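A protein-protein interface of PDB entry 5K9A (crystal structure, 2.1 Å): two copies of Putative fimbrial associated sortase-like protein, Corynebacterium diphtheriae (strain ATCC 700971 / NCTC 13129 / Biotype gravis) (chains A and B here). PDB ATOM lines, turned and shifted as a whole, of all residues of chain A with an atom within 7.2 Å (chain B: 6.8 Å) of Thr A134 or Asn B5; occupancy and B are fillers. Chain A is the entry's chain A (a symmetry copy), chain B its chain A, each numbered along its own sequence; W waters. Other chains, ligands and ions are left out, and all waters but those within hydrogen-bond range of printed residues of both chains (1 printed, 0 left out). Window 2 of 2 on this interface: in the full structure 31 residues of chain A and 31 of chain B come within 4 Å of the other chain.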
ATOM      1  N   ILE A  86      -1.230  37.751   6.543  1.00  0.00           N
ATOM      2  CA  ILE A  86      -1.312  37.649   8.010  1.00  0.00           C
ATOM      3  C   ILE A  86      -0.031  37.089   8.609  1.00  0.00           C
ATOM      4  O   ILE A  86      -0.023  36.580   9.722  1.00  0.00           O
ATOM      5  CB  ILE A  86      -2.525  36.825   8.439  1.00  0.00           C
ATOM      6  CG1 ILE A  86      -2.500  35.429   7.843  1.00  0.00           C
ATOM      7  CG2 ILE A  86      -3.796  37.577   7.988  1.00  0.00           C
ATOM      8  CD1 ILE A  86      -3.575  34.523   8.400  1.00  0.00           C
ATOM      9  N   ASP A  87       1.022  37.091   7.800  1.00  0.00           N
ATOM     10  CA  ASP A  87       2.339  36.615   8.207  1.00  0.00           C
ATOM     11  C   ASP A  87       2.284  35.205   8.800  1.00  0.00           C
ATOM     12  O   ASP A  87       2.911  34.924   9.826  1.00  0.00           O
ATOM     13  CB  ASP A  87       2.955  37.604   9.234  1.00  0.00           C
ATOM     14  CG  ASP A  87       4.479  37.430   9.413  1.00  0.00           C
ATOM     15  OD1 ASP A  87       5.174  36.922   8.505  1.00  0.00           O
ATOM     16  OD2 ASP A  87       4.997  37.826  10.472  1.00  0.00           O
ATOM     17  N   ALA A  88       1.548  34.297   8.172  1.00  0.00           N
ATOM     18  CA  ALA A  88       1.488  32.929   8.642  1.00  0.00           C
ATOM     19  C   ALA A  88       2.298  32.028   7.730  1.00  0.00           C
ATOM     20  O   ALA A  88       2.219  32.113   6.473  1.00  0.00           O
ATOM     21  CB  ALA A  88       0.056  32.438   8.718  1.00  0.00           C
ATOM     22  N   HIS A  89       3.091  31.174   8.364  1.00  0.00           N
ATOM     23  CA  HIS A  89       3.882  30.191   7.664  1.00  0.00           C
ATOM     24  C   HIS A  89       3.928  28.919   8.503  1.00  0.00           C
ATOM     25  O   HIS A  89       4.592  28.888   9.550  1.00  0.00           O
ATOM     26  CB  HIS A  89       5.285  30.730   7.436  1.00  0.00           C
ATOM     27  CG  HIS A  89       6.060  29.919   6.445  1.00  0.00           C
ATOM     28  ND1 HIS A  89       7.431  29.939   6.382  1.00  0.00           N
ATOM     29  CD2 HIS A  89       5.659  29.001   5.536  1.00  0.00           C
ATOM     30  CE1 HIS A  89       7.837  29.116   5.420  1.00  0.00           C
ATOM     31  NE2 HIS A  89       6.781  28.549   4.885  1.00  0.00           N
ATOM     32  N   LEU A  90       3.232  27.878   8.048  1.00  0.00           N
ATOM     33  CA  LEU A  90       2.947  26.769   8.909  1.00  0.00           C
ATOM     34  C   LEU A  90       3.006  25.460   8.188  1.00  0.00           C
ATOM     35  O   LEU A  90       2.705  25.381   6.990  1.00  0.00           O
ATOM     36  CB  LEU A  90       1.544  26.919   9.478  1.00  0.00           C
ATOM     37  CG  LEU A  90       1.316  28.102  10.442  1.00  0.00           C
ATOM     38  CD1 LEU A  90      -0.153  28.332  10.695  1.00  0.00           C
ATOM     39  CD2 LEU A  90       2.072  27.965  11.744  1.00  0.00           C
ATOM     40  N   GLY A 126      -6.966  24.600  11.309  1.00  0.00           N
ATOM     41  CA  GLY A 126      -6.099  25.104  12.398  1.00  0.00           C
ATOM     42  C   GLY A 126      -6.898  25.638  13.555  1.00  0.00           C
ATOM     43  O   GLY A 126      -8.013  26.140  13.394  1.00  0.00           O
ATOM     44  N   HIS A 127      -6.334  25.535  14.731  1.00  0.00           N
ATOM     45  CA  HIS A 127      -6.928  26.140  15.914  1.00  0.00           C
ATOM     46  C   HIS A 127      -6.832  27.652  15.866  1.00  0.00           C
ATOM     47  O   HIS A 127      -5.971  28.251  15.255  1.00  0.00           O
ATOM     48  CB  HIS A 127      -6.157  25.765  17.164  1.00  0.00           C
ATOM     49  CG  HIS A 127      -6.457  24.436  17.734  1.00  0.00           C
ATOM     50  ND1 HIS A 127      -7.731  24.014  18.014  1.00  0.00           N
ATOM     51  CD2 HIS A 127      -5.624  23.460  18.194  1.00  0.00           C
ATOM     52  CE1 HIS A 127      -7.697  22.806  18.543  1.00  0.00           C
ATOM     53  NE2 HIS A 127      -6.425  22.450  18.688  1.00  0.00           N
ATOM     54  N   SER A 128      -7.756  28.242  16.553  1.00  0.00           N
ATOM     55  CA  SER A 128      -7.597  29.595  16.973  1.00  0.00           C
ATOM     56  C   SER A 128      -7.785  29.527  18.494  1.00  0.00           C
ATOM     57  O   SER A 128      -8.482  28.661  19.030  1.00  0.00           O
ATOM     58  CB  SER A 128      -8.630  30.489  16.331  1.00  0.00           C
ATOM     59  OG  SER A 128      -9.870  29.837  16.345  1.00  0.00           O
ATOM     60  N   GLY A 129      -7.124  30.386  19.198  1.00  0.00           N
ATOM     61  CA  GLY A 129      -7.254  30.394  20.660  1.00  0.00           C
ATOM     62  C   GLY A 129      -6.403  29.367  21.438  1.00  0.00           C
ATOM     63  O   GLY A 129      -6.590  29.184  22.653  1.00  0.00           O
ATOM     64  N   LEU A 130      -5.459  28.703  20.800  1.00  0.00           N
ATOM     65  CA  LEU A 130      -4.602  27.790  21.563  1.00  0.00           C
ATOM     66  C   LEU A 130      -3.552  28.651  22.326  1.00  0.00           C
ATOM     67  O   LEU A 130      -2.950  29.544  21.742  1.00  0.00           O
ATOM     68  CB  LEU A 130      -3.971  26.752  20.619  1.00  0.00           C
ATOM     69  CG  LEU A 130      -3.188  25.606  21.223  1.00  0.00           C
ATOM     70  CD1 LEU A 130      -4.140  24.548  21.755  1.00  0.00           C
ATOM     71  CD2 LEU A 130      -2.276  24.948  20.188  1.00  0.00           C
ATOM     72  N   ALA A 131      -3.335  28.395  23.626  1.00  0.00           N
ATOM     73  CA  ALA A 131      -2.323  29.099  24.374  1.00  0.00           C
ATOM     74  C   ALA A 131      -0.962  28.823  23.707  1.00  0.00           C
ATOM     75  O   ALA A 131      -0.671  27.678  23.294  1.00  0.00           O
ATOM     76  CB  ALA A 131      -2.258  28.556  25.783  1.00  0.00           C
ATOM     77  N   ASN A 132      -0.126  29.832  23.636  1.00  0.00           N
ATOM     78  CA  ASN A 132       1.251  29.610  23.161  1.00  0.00           C
ATOM     79  C   ASN A 132       1.525  29.100  21.677  1.00  0.00           C
ATOM     80  O   ASN A 132       2.601  28.587  21.394  1.00  0.00           O
ATOM     81  CB  ASN A 132       2.041  28.704  24.184  1.00  0.00           C
ATOM     82  CG  ASN A 132       1.891  29.155  25.663  1.00  0.00           C
ATOM     83  OD1 ASN A 132       1.694  30.344  25.975  1.00  0.00           O
ATOM     84  ND2 ASN A 132       1.967  28.181  26.578  1.00  0.00           N
ATOM     85  N   ALA A 133       0.551  29.205  20.771  1.00  0.00           N
ATOM     86  CA  ALA A 133       0.831  29.253  19.331  1.00  0.00           C
ATOM     87  C   ALA A 133      -0.288  29.970  18.625  1.00  0.00           C
ATOM     88  O   ALA A 133      -1.466  29.761  18.909  1.00  0.00           O
ATOM     89  CB  ALA A 133       1.029  27.882  18.774  1.00  0.00           C
ATOM     90  N   THR A 134       0.083  30.852  17.729  1.00  0.00           N
ATOM     91  CA  THR A 134      -0.853  31.647  16.982  1.00  0.00           C
ATOM     92  C   THR A 134      -1.690  30.828  16.010  1.00  0.00           C
ATOM     93  O   THR A 134      -2.906  31.044  15.929  1.00  0.00           O
ATOM     94  CB  THR A 134      -0.085  32.721  16.247  1.00  0.00           C
ATOM     95  OG1 THR A 134       0.497  33.557  17.257  1.00  0.00           O
ATOM     96  CG2 THR A 134      -0.988  33.571  15.362  1.00  0.00           C
ATOM     97  N   LEU A 135      -1.063  29.913  15.267  1.00  0.00           N
ATOM     98  CA  LEU A 135      -1.796  29.065  14.317  1.00  0.00           C
ATOM     99  C   LEU A 135      -2.747  29.864  13.401  1.00  0.00           C
ATOM    100  O   LEU A 135      -2.295  30.761  12.724  1.00  0.00           O
ATOM    101  CB  LEU A 135      -2.496  27.897  15.043  1.00  0.00           C
ATOM    102  CG  LEU A 135      -1.442  27.001  15.732  1.00  0.00           C
ATOM    103  CD1 LEU A 135      -2.028  26.133  16.839  1.00  0.00           C
ATOM    104  CD2 LEU A 135      -0.760  26.130  14.707  1.00  0.00           C
ATOM    105  N   PHE A 136      -4.044  29.598  13.440  1.00  0.00           N
ATOM    106  CA  PHE A 136      -5.019  30.343  12.661  1.00  0.00           C
ATOM    107  C   PHE A 136      -5.775  31.454  13.469  1.00  0.00           C
ATOM    108  O   PHE A 136      -6.852  31.867  13.054  1.00  0.00           O
ATOM    109  CB  PHE A 136      -6.087  29.387  12.011  1.00  0.00           C
ATOM    110  CG  PHE A 136      -5.711  28.768  10.698  1.00  0.00           C
ATOM    111  CD1 PHE A 136      -4.592  29.157   9.980  1.00  0.00           C
ATOM    112  CD2 PHE A 136      -6.507  27.776  10.158  1.00  0.00           C
ATOM    113  CE1 PHE A 136      -4.272  28.555   8.780  1.00  0.00           C
ATOM    114  CE2 PHE A 136      -6.194  27.176   8.950  1.00  0.00           C
ATOM    115  CZ  PHE A 136      -5.082  27.569   8.246  1.00  0.00           C
ATOM    116  N   ASP A 137      -5.198  31.975  14.561  1.00  0.00           N
ATOM    117  CA  ASP A 137      -5.781  33.116  15.250  1.00  0.00           C
ATOM    118  C   ASP A 137      -6.091  34.290  14.317  1.00  0.00           C
ATOM    119  O   ASP A 137      -7.078  34.990  14.565  1.00  0.00           O
ATOM    120  CB  ASP A 137      -4.837  33.672  16.322  1.00  0.00           C
ATOM    121  CG  ASP A 137      -4.744  32.789  17.536  1.00  0.00           C
ATOM    122  OD1 ASP A 137      -5.585  31.843  17.658  1.00  0.00           O
ATOM    123  OD2 ASP A 137      -3.804  33.033  18.367  1.00  0.00           O
ATOM    124  N   ASN A 138      -5.253  34.523  13.301  1.00  0.00           N
ATOM    125  CA  ASN A 138      -5.471  35.660  12.403  1.00  0.00           C
ATOM    126  C   ASN A 138      -6.154  35.361  11.067  1.00  0.00           C
ATOM    127  O   ASN A 138      -6.261  36.239  10.185  1.00  0.00           O
ATOM    128  CB  ASN A 138      -4.191  36.408  12.164  1.00  0.00           C
ATOM    129  CG  ASN A 138      -3.612  36.939  13.469  1.00  0.00           C
ATOM    130  OD1 ASN A 138      -4.296  37.518  14.260  1.00  0.00           O
ATOM    131  ND2 ASN A 138      -2.415  36.666  13.694  1.00  0.00           N
ATOM    132  N   LEU A 139      -6.704  34.160  10.935  1.00  0.00           N
ATOM    133  CA  LEU A 139      -7.399  33.812   9.676  1.00  0.00           C
ATOM    134  C   LEU A 139      -8.548  34.800   9.401  1.00  0.00           C
ATOM    135  O   LEU A 139      -8.828  35.140   8.257  1.00  0.00           O
ATOM    136  CB  LEU A 139      -7.934  32.400   9.738  1.00  0.00           C
ATOM    137  CG  LEU A 139      -8.519  31.835   8.465  1.00  0.00           C
ATOM    138  CD1 LEU A 139      -7.426  31.823   7.423  1.00  0.00           C
ATOM    139  CD2 LEU A 139      -9.008  30.433   8.730  1.00  0.00           C
ATOM    140  N   SER B   1       3.991  30.990  23.004  1.00  0.00           N
ATOM    141  CA  SER B   1       5.170  31.867  22.991  1.00  0.00           C
ATOM    142  C   SER B   1       5.533  32.194  21.537  1.00  0.00           C
ATOM    143  O   SER B   1       5.148  31.471  20.590  1.00  0.00           O
ATOM    144  CB  SER B   1       6.315  31.166  23.706  1.00  0.00           C
ATOM    145  OG  SER B   1       6.440  29.852  23.207  1.00  0.00           O
ATOM    146  N   ASN B   2       6.240  33.313  21.372  1.00  0.00           N
ATOM    147  CA  ASN B   2       6.947  33.604  20.126  1.00  0.00           C
ATOM    148  C   ASN B   2       7.858  32.442  19.766  1.00  0.00           C
ATOM    149  O   ASN B   2       8.043  32.201  18.600  1.00  0.00           O
ATOM    150  CB  ASN B   2       7.822  34.856  20.236  1.00  0.00           C
ATOM    151  CG  ASN B   2       7.023  36.119  20.452  1.00  0.00           C
ATOM    152  OD1 ASN B   2       5.821  36.174  20.190  1.00  0.00           O
ATOM    153  ND2 ASN B   2       7.698  37.154  20.922  1.00  0.00           N
ATOM    154  N   ALA B   3       8.417  31.761  20.778  1.00  0.00           N
ATOM    155  CA  ALA B   3       9.328  30.635  20.595  1.00  0.00           C
ATOM    156  C   ALA B   3       8.630  29.493  19.811  1.00  0.00           C
ATOM    157  O   ALA B   3       9.203  28.898  18.909  1.00  0.00           O
ATOM    158  CB  ALA B   3       9.801  30.119  21.948  1.00  0.00           C
ATOM    159  N   ASN B   4       7.413  29.175  20.224  1.00  0.00           N
ATOM    160  CA  ASN B   4       6.609  28.189  19.538  1.00  0.00           C
ATOM    161  C   ASN B   4       6.220  28.552  18.111  1.00  0.00           C
ATOM    162  O   ASN B   4       6.285  27.719  17.242  1.00  0.00           O
ATOM    163  CB  ASN B   4       5.349  27.970  20.287  1.00  0.00           C
ATOM    164  CG  ASN B   4       5.110  26.544  20.540  1.00  0.00           C
ATOM    165  OD1 ASN B   4       5.174  25.704  19.643  1.00  0.00           O
ATOM    166  ND2 ASN B   4       4.875  26.237  21.789  1.00  0.00           N
ATOM    167  N   ASN B   5       5.829  29.791  17.890  1.00  0.00           N
ATOM    168  CA  ASN B   5       5.505  30.280  16.570  1.00  0.00           C
ATOM    169  C   ASN B   5       6.711  30.179  15.677  1.00  0.00           C
ATOM    170  O   ASN B   5       6.637  29.668  14.558  1.00  0.00           O
ATOM    171  CB  ASN B   5       5.012  31.713  16.584  1.00  0.00           C
ATOM    172  CG  ASN B   5       3.652  31.844  17.236  1.00  0.00           C
ATOM    173  OD1 ASN B   5       2.878  30.901  17.319  1.00  0.00           O
ATOM    174  ND2 ASN B   5       3.359  33.040  17.723  1.00  0.00           N
ATOM    175  N   ALA B   6       7.839  30.641  16.181  1.00  0.00           N
ATOM    176  CA  ALA B   6       9.055  30.562  15.421  1.00  0.00           C
ATOM    177  C   ALA B   6       9.412  29.108  15.137  1.00  0.00           C
ATOM    178  O   ALA B   6       9.848  28.830  14.023  1.00  0.00           O
ATOM    179  CB  ALA B   6      10.181  31.267  16.133  1.00  0.00           C
ATOM    180  N   ARG B   7       9.259  28.224  16.104  1.00  0.00           N
ATOM    181  CA  ARG B   7       9.513  26.817  15.895  1.00  0.00           C
ATOM    182  C   ARG B   7       8.636  26.198  14.769  1.00  0.00           C
ATOM    183  O   ARG B   7       9.130  25.474  13.937  1.00  0.00           O
ATOM    184  CB  ARG B   7       9.318  26.045  17.194  1.00  0.00           C
ATOM    185  CG  ARG B   7       9.682  24.583  17.113  1.00  0.00           C
ATOM    186  CD  ARG B   7      10.184  23.909  18.444  1.00  0.00           C
ATOM    187  NE  ARG B   7       9.330  24.225  19.549  1.00  0.00           N
ATOM    188  CZ  ARG B   7       9.618  25.065  20.527  1.00  0.00           C
ATOM    189  NH1 ARG B   7      10.794  25.655  20.604  1.00  0.00           N
ATOM    190  NH2 ARG B   7       8.700  25.314  21.442  1.00  0.00           N
ATOM    191  N   GLN B   8       7.347  26.529  14.768  1.00  0.00           N
ATOM    192  CA  GLN B   8       6.416  26.053  13.729  1.00  0.00           C
ATOM    193  C   GLN B   8       6.764  26.581  12.372  1.00  0.00           C
ATOM    194  O   GLN B   8       6.824  25.770  11.432  1.00  0.00           O
ATOM    195  CB  GLN B   8       4.999  26.342  14.116  1.00  0.00           C
ATOM    196  CG  GLN B   8       4.638  25.492  15.305  1.00  0.00           C
ATOM    197  CD  GLN B   8       3.286  25.861  15.861  1.00  0.00           C
ATOM    198  OE1 GLN B   8       2.627  26.740  15.347  1.00  0.00           O
ATOM    199  NE2 GLN B   8       2.891  25.195  16.933  1.00  0.00           N
ATOM    200  N   ALA B   9       7.084  27.874  12.263  1.00  0.00           N
ATOM    201  CA  ALA B   9       7.520  28.467  11.040  1.00  0.00           C
ATOM    202  C   ALA B   9       8.815  27.844  10.500  1.00  0.00           C
ATOM    203  O   ALA B   9       8.982  27.636   9.271  1.00  0.00           O
ATOM    204  CB  ALA B   9       7.720  29.957  11.200  1.00  0.00           C
ATOM    205  N   ARG B  10       9.756  27.519  11.394  1.00  0.00           N
ATOM    206  CA  ARG B  10      10.964  26.909  10.984  1.00  0.00           C
ATOM    207  C   ARG B  10      10.740  25.451  10.484  1.00  0.00           C
ATOM    208  O   ARG B  10      11.425  25.010   9.580  1.00  0.00           O
ATOM    209  CB  ARG B  10      11.987  26.954  12.132  1.00  0.00           C
ATOM    210  CG  ARG B  10      13.363  26.468  11.707  1.00  0.00           C
ATOM    211  CD  ARG B  10      14.420  26.754  12.775  1.00  0.00           C
ATOM    212  NE  ARG B  10      15.767  26.507  12.247  1.00  0.00           N
ATOM    213  CZ  ARG B  10      16.892  26.479  12.969  1.00  0.00           C
ATOM    214  NH1 ARG B  10      18.037  26.228  12.360  1.00  0.00           N
ATOM    215  NH2 ARG B  10      16.875  26.670  14.287  1.00  0.00           N
HETATM  216  O   HOH W   1       1.835  29.257  15.162  1.00  0.00           O
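Water W1 lies within hydrogen-bond range of the side-chain amide oxygen (OE1) of Gln B8 (2.6 Å), the side-chain amide oxygen (OD1) of Asn B5 (2.9 Å), the backbone NH (N) of Leu A135 (3.0 Å) and the backbone NH (N) of Thr A134 (3.5 Å).
Among the printed residues, merely in contact across the chains: Ala A133 with Asn B5 (3.3 Å), His A89 with Ala B9 (3.3 Å), Leu A135 with Gln B8 (3.5 Å), Ala A133 with Gln B8 (3.8 Å) and Leu A90 with Gln B8 (3.8 Å).
N of Ser B1 lies close to O of Asn A132, at 3.2 Å. The side-chain amide nitrogen (ND2) of Asn B4 lies close to the backbone carbonyl oxygen (O) of Asn A132 (3.3 Å). OD1 of Asn B5 lies within hydrogen-bond range of N of Thr A134, 2.8 Å away.
No position is printed for both chains. Of the 8 pairs that touch across the chains among the printed residues, none has its exchanged pair printed and touching as well.
Of the printed residues of chain B, Thr A134 touches Asn B5 (2.8 Å). Of chain A, only Ala A133 (3.3 Å) and Thr A134 (2.8 Å) come within 4 Å of Asn B5. Of the printed residues of chain A, Asn B4 touches Asn A132 (3.0 Å). Of the printed residues of chain A, Ala B9 touches His A89 (3.3 Å). Of the printed residues of chain B, Leu A135 touches Gln B8. Printed residues of chain B within 4 Å of Asn A132: Ser B1 (3.1 Å) and Asn B4 (3.0 Å). Printed residues of chain B within 4 Å of Ala A133: Asn B5 (3.3 Å) and Gln B8 (3.8 Å). Leu A130 touches none of the printed residues of chain B. The nearest residue of chain B that does not touch Thr A134 is Gln B8 (5.4 Å). The nearest printed residue of chain B that does not touch His A89 is Gln B8 (4.2 Å).
Of the 19 printed residues of chain A, 6 touch a printed residue of chain B. Printed residues of chain A that touch a printed residue of chain B: His A89, Leu A90, Asn A132, Ala A133, Thr A134 and Leu A135. Hydrophobic or aromatic side chains of chain A within 4 Å of the printed part of chain B: Leu A90, Ala A133 and Leu A135. Of the 10 printed residues of chain B, 5 touch a printed residue of chain A. Hydrophobic or aromatic side chains of chain B within 4 Å of the printed part of chain A: Ala B9. Among the printed residues, no Asp or Glu carboxylate lies within 4 Å of a Lys or Arg side-chain nitrogen of the other chain.
The side-chain hydroxyl (OG) of Ser B1 is in hydrogen-bond range of the backbone NH (N) of Asn B4 (3.2 Å).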
